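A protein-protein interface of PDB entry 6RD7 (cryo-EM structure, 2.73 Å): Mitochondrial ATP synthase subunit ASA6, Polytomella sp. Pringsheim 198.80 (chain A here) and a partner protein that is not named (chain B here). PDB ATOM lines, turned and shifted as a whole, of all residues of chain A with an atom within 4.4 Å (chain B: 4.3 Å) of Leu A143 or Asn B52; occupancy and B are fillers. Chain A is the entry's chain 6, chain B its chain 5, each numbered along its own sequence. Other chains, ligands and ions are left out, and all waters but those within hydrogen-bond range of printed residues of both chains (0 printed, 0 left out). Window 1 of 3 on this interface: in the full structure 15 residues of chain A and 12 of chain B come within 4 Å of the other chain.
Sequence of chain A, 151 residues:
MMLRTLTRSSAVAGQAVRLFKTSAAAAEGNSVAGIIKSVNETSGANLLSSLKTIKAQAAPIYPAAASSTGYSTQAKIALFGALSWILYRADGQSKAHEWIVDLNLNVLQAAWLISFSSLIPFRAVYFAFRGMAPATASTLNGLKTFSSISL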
ATOM      1  N   GLY A 142      18.239   1.382  29.824  1.00  0.00           N
ATOM      2  CA  GLY A 142      17.797   2.284  28.788  1.00  0.00           C
ATOM      3  C   GLY A 142      17.112   3.514  29.329  1.00  0.00           C
ATOM      4  O   GLY A 142      17.697   4.294  30.085  1.00  0.00           O
ATOM      5  N   LEU A 143      15.886   3.716  28.853  1.00  0.00           N
ATOM      6  CA  LEU A 143      15.001   4.769  29.328  1.00  0.00           C
ATOM      7  C   LEU A 143      14.811   4.724  30.841  1.00  0.00           C
ATOM      8  O   LEU A 143      14.409   3.707  31.407  1.00  0.00           O
ATOM      9  CB  LEU A 143      13.654   4.627  28.627  1.00  0.00           C
ATOM     10  CG  LEU A 143      12.478   5.440  29.141  1.00  0.00           C
ATOM     11  CD1 LEU A 143      12.787   6.863  28.922  1.00  0.00           C
ATOM     12  CD2 LEU A 143      11.211   5.070  28.410  1.00  0.00           C
ATOM     13  N   LYS A 144      15.115   5.839  31.494  1.00  0.00           N
ATOM     14  CA  LYS A 144      14.870   6.016  32.914  1.00  0.00           C
ATOM     15  C   LYS A 144      13.511   6.665  33.111  1.00  0.00           C
ATOM     16  O   LYS A 144      12.963   7.281  32.196  1.00  0.00           O
ATOM     17  CB  LYS A 144      15.950   6.879  33.565  1.00  0.00           C
ATOM     18  CG  LYS A 144      17.328   6.268  33.560  1.00  0.00           C
ATOM     19  CD  LYS A 144      17.336   4.927  34.252  1.00  0.00           C
ATOM     20  CE  LYS A 144      18.675   4.248  34.083  1.00  0.00           C
ATOM     21  NZ  LYS A 144      19.153   4.332  32.677  1.00  0.00           N
ATOM     22  N   THR A 145      12.972   6.529  34.322  1.00  0.00           N
ATOM     23  CA  THR A 145      11.630   7.032  34.587  1.00  0.00           C
ATOM     24  C   THR A 145      11.612   8.555  34.660  1.00  0.00           C
ATOM     25  O   THR A 145      10.707   9.194  34.114  1.00  0.00           O
ATOM     26  CB  THR A 145      11.097   6.413  35.878  1.00  0.00           C
ATOM     27  OG1 THR A 145      11.010   4.993  35.728  1.00  0.00           O
ATOM     28  CG2 THR A 145       9.721   6.949  36.222  1.00  0.00           C
ATOM     29  N   SER A 147      13.233  10.873  33.198  1.00  0.00           N
ATOM     30  CA  SER A 147      13.267  11.627  31.950  1.00  0.00           C
ATOM     31  C   SER A 147      11.921  11.584  31.241  1.00  0.00           C
ATOM     32  O   SER A 147      11.571  12.510  30.503  1.00  0.00           O
ATOM     33  CB  SER A 147      14.365  11.094  31.038  1.00  0.00           C
ATOM     34  OG  SER A 147      14.082   9.774  30.631  1.00  0.00           O
ATOM     35  N   SER A 148      11.154  10.520  31.452  1.00  0.00           N
ATOM     36  CA  SER A 148       9.894  10.314  30.757  1.00  0.00           C
ATOM     37  C   SER A 148       8.680  10.563  31.640  1.00  0.00           C
ATOM     38  O   SER A 148       7.597  10.057  31.335  1.00  0.00           O
ATOM     39  CB  SER A 148       9.833   8.897  30.191  1.00  0.00           C
ATOM     40  OG  SER A 148       9.696   7.948  31.231  1.00  0.00           O
ATOM     41  N   TRP B  44      20.415   0.318  23.230  1.00  0.00           N
ATOM     42  CA  TRP B  44      19.900   0.943  24.443  1.00  0.00           C
ATOM     43  C   TRP B  44      21.021   1.266  25.421  1.00  0.00           C
ATOM     44  O   TRP B  44      21.012   2.329  26.050  1.00  0.00           O
ATOM     45  CB  TRP B  44      18.853   0.048  25.096  1.00  0.00           C
ATOM     46  CG  TRP B  44      17.454   0.304  24.627  1.00  0.00           C
ATOM     47  CD1 TRP B  44      16.644  -0.570  23.975  1.00  0.00           C
ATOM     48  CD2 TRP B  44      16.696   1.510  24.784  1.00  0.00           C
ATOM     49  NE1 TRP B  44      15.433   0.011  23.710  1.00  0.00           N
ATOM     50  CE2 TRP B  44      15.440   1.289  24.198  1.00  0.00           C
ATOM     51  CE3 TRP B  44      16.959   2.757  25.359  1.00  0.00           C
ATOM     52  CZ2 TRP B  44      14.451   2.261  24.172  1.00  0.00           C
ATOM     53  CZ3 TRP B  44      15.980   3.718  25.331  1.00  0.00           C
ATOM     54  CH2 TRP B  44      14.740   3.467  24.744  1.00  0.00           C
ATOM     55  N   ALA B  48      21.612   5.177  26.314  1.00  0.00           N
ATOM     56  CA  ALA B  48      20.900   5.495  27.552  1.00  0.00           C
ATOM     57  C   ALA B  48      21.168   6.919  28.025  1.00  0.00           C
ATOM     58  O   ALA B  48      20.226   7.665  28.315  1.00  0.00           O
ATOM     59  CB  ALA B  48      21.277   4.492  28.638  1.00  0.00           C
ATOM     60  N   LYS B  49      22.434   7.340  28.013  1.00  0.00           N
ATOM     61  CA  LYS B  49      22.803   8.661  28.510  1.00  0.00           C
ATOM     62  C   LYS B  49      22.272   9.773  27.609  1.00  0.00           C
ATOM     63  O   LYS B  49      21.596  10.695  28.083  1.00  0.00           O
ATOM     64  CB  LYS B  49      24.323   8.745  28.648  1.00  0.00           C
ATOM     65  CG  LYS B  49      24.821   9.913  29.468  1.00  0.00           C
ATOM     66  CD  LYS B  49      25.463  10.962  28.579  1.00  0.00           C
ATOM     67  CE  LYS B  49      25.764  12.232  29.348  1.00  0.00           C
ATOM     68  NZ  LYS B  49      26.105  13.354  28.431  1.00  0.00           N
ATOM     69  N   ARG B  50      22.537   9.685  26.301  1.00  0.00           N
ATOM     70  CA  ARG B  50      22.100  10.724  25.370  1.00  0.00           C
ATOM     71  C   ARG B  50      20.587  10.740  25.214  1.00  0.00           C
ATOM     72  O   ARG B  50      19.984  11.807  25.080  1.00  0.00           O
ATOM     73  CB  ARG B  50      22.742  10.525  24.002  1.00  0.00           C
ATOM     74  CG  ARG B  50      24.219  10.750  23.933  1.00  0.00           C
ATOM     75  CD  ARG B  50      24.681  10.403  22.542  1.00  0.00           C
ATOM     76  NE  ARG B  50      24.415  11.478  21.600  1.00  0.00           N
ATOM     77  CZ  ARG B  50      25.355  12.273  21.108  1.00  0.00           C
ATOM     78  NH1 ARG B  50      25.031  13.239  20.260  1.00  0.00           N
ATOM     79  NH2 ARG B  50      26.620  12.094  21.459  1.00  0.00           N
ATOM     80  N   TYR B  51      19.962   9.563  25.215  1.00  0.00           N
ATOM     81  CA  TYR B  51      18.520   9.443  25.090  1.00  0.00           C
ATOM     82  C   TYR B  51      17.818  10.045  26.293  1.00  0.00           C
ATOM     83  O   TYR B  51      16.854  10.801  26.139  1.00  0.00           O
ATOM     84  CB  TYR B  51      18.171   7.964  24.927  1.00  0.00           C
ATOM     85  CG  TYR B  51      16.724   7.620  24.688  1.00  0.00           C
ATOM     86  CD1 TYR B  51      16.239   7.465  23.402  1.00  0.00           C
ATOM     87  CD2 TYR B  51      15.859   7.389  25.749  1.00  0.00           C
ATOM     88  CE1 TYR B  51      14.927   7.130  23.179  1.00  0.00           C
ATOM     89  CE2 TYR B  51      14.547   7.063  25.535  1.00  0.00           C
ATOM     90  CZ  TYR B  51      14.088   6.930  24.250  1.00  0.00           C
ATOM     91  OH  TYR B  51      12.779   6.593  24.040  1.00  0.00           O
ATOM     92  N   ASN B  52      18.306   9.742  27.497  1.00  0.00           N
ATOM     93  CA  ASN B  52      17.692  10.289  28.694  1.00  0.00           C
ATOM     94  C   ASN B  52      17.947  11.782  28.809  1.00  0.00           C
ATOM     95  O   ASN B  52      17.077  12.523  29.270  1.00  0.00           O
ATOM     96  CB  ASN B  52      18.209   9.546  29.916  1.00  0.00           C
ATOM     97  CG  ASN B  52      17.540   8.213  30.099  1.00  0.00           C
ATOM     98  OD1 ASN B  52      16.326   8.097  29.972  1.00  0.00           O
ATOM     99  ND2 ASN B  52      18.326   7.193  30.398  1.00  0.00           N
ATOM    100  N   GLU B  53      19.102  12.256  28.332  1.00  0.00           N
ATOM    101  CA  GLU B  53      19.376  13.689  28.365  1.00  0.00           C
ATOM    102  C   GLU B  53      18.511  14.449  27.365  1.00  0.00           C
ATOM    103  O   GLU B  53      17.972  15.516  27.682  1.00  0.00           O
ATOM    104  CB  GLU B  53      20.857  13.939  28.097  1.00  0.00           C
ATOM    105  CG  GLU B  53      21.247  15.403  28.097  1.00  0.00           C
ATOM    106  CD  GLU B  53      21.035  16.064  29.443  1.00  0.00           C
ATOM    107  OE1 GLU B  53      21.367  15.440  30.472  1.00  0.00           O
ATOM    108  OE2 GLU B  53      20.534  17.206  29.477  1.00  0.00           O
ATOM    109  N   LYS B  54      18.345  13.902  26.159  1.00  0.00           N
ATOM    110  CA  LYS B  54      17.523  14.550  25.142  1.00  0.00           C
ATOM    111  C   LYS B  54      16.053  14.534  25.531  1.00  0.00           C
ATOM    112  O   LYS B  54      15.336  15.525  25.336  1.00  0.00           O
ATOM    113  CB  LYS B  54      17.737  13.856  23.798  1.00  0.00           C
ATOM    114  CG  LYS B  54      16.801  14.290  22.698  1.00  0.00           C
ATOM    115  CD  LYS B  54      17.213  13.717  21.365  1.00  0.00           C
ATOM    116  CE  LYS B  54      16.640  14.542  20.233  1.00  0.00           C
ATOM    117  NZ  LYS B  54      16.409  13.730  19.012  1.00  0.00           N
ATOM    118  N   LEU B  55      15.598  13.431  26.122  1.00  0.00           N
ATOM    119  CA  LEU B  55      14.220  13.348  26.580  1.00  0.00           C
ATOM    120  C   LEU B  55      13.993  14.229  27.800  1.00  0.00           C
ATOM    121  O   LEU B  55      12.896  14.764  27.990  1.00  0.00           O
ATOM    122  CB  LEU B  55      13.883  11.892  26.881  1.00  0.00           C
ATOM    123  CG  LEU B  55      12.456  11.578  27.283  1.00  0.00           C
ATOM    124  CD1 LEU B  55      11.543  12.015  26.197  1.00  0.00           C
ATOM    125  CD2 LEU B  55      12.334  10.123  27.458  1.00  0.00           C
ATOM    126  N   PHE B  56      15.023  14.406  28.626  1.00  0.00           N
ATOM    127  CA  PHE B  56      14.938  15.315  29.760  1.00  0.00           C
ATOM    128  C   PHE B  56      14.862  16.762  29.299  1.00  0.00           C
ATOM    129  O   PHE B  56      14.169  17.581  29.911  1.00  0.00           O
ATOM    130  CB  PHE B  56      16.149  15.088  30.660  1.00  0.00           C
ATOM    131  CG  PHE B  56      16.183  15.953  31.872  1.00  0.00           C
ATOM    132  CD1 PHE B  56      15.334  15.708  32.931  1.00  0.00           C
ATOM    133  CD2 PHE B  56      17.086  16.993  31.967  1.00  0.00           C
ATOM    134  CE1 PHE B  56      15.368  16.500  34.053  1.00  0.00           C
ATOM    135  CE2 PHE B  56      17.127  17.783  33.090  1.00  0.00           C
ATOM    136  CZ  PHE B  56      16.268  17.534  34.133  1.00  0.00           C
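The side-chain amide nitrogen (ND2) of Asn B52 is in hydrogen-bond range of the backbone carbonyl oxygen (O) of Gly A142 (3.0 Å). The side-chain hydroxyl (OG) of Ser A147 sits at hydrogen-bond distance from the side-chain amide oxygen (OD1) of Asn B52 (2.9 Å). The side-chain amide oxygen (OD1) of Asn B52 sits at hydrogen-bond distance from the backbone NH (N) of Lys A144 (3.0 Å).
The backbone carbonyl oxygen (O) of Lys A144 is in hydrogen-bond range of the side-chain hydroxyl (OG) of Ser A148. The backbone carbonyl oxygen (O) of Ala B48 is in hydrogen-bond range of the side-chain amide nitrogen (ND2) of Asn B52 (2.9 Å). O of Lys A144 is in hydrogen-bond range of OG of Ser A147. O of Thr A145 sits at hydrogen-bond distance from OG of Ser A148 (3.3 Å). NZ of Lys A144 sits at hydrogen-bond distance from O of Gly A142 (3.0 Å).
Gly A142 touches Trp B44 (CA to CE3, 3.6 Å). Ala B48 touches Gly A142 (CB to O, 3.9 Å). Leu A143 touches Trp B44. CD1 of Leu A143 touches CE2 of Tyr B51, at 3.8 Å. Leu A143 touches Asn B52. Leu A143 touches Leu B55. Leu B55 touches Ser A147 (CG to O, 3.5 Å). CB of Ser A148 touches CD2 of Leu B55, at 3.9 Å.
Printed residues of chain B within 4 Å of Ser A148: Leu B55. Of the printed residues of chain A, Trp B44 touches Gly A142 (3.6 Å) and Leu A143 (3.5 Å). Printed residues of chain A within 4 Å of Ala B48: Gly A142 (3.9 Å). Of the printed residues of chain A, Tyr B51 touches Leu A143. Of the printed residues of chain A, Leu B55 touches Leu A143, Ser A147 and Ser A148.
Of the 6 printed residues of chain A, 5 touch a printed residue of chain B. Hydrophobic or aromatic side chains of chain A within 4 Å of the printed part of chain B: Leu A143. Printed residues of chain B that touch a printed residue of chain A: Trp B44, Ala B48, Tyr B51, Asn B52 and Leu B55. Hydrophobic or aromatic side chains of chain B within 4 Å of the printed part of chain A: Trp B44, Ala B48, Tyr B51 and Leu B55. Among the printed residues, 11 pairs touch across the chains. Among the printed residues, no Asp or Glu carboxylate lies within 4 Å of a Lys or Arg side-chain nitrogen of the other chain.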
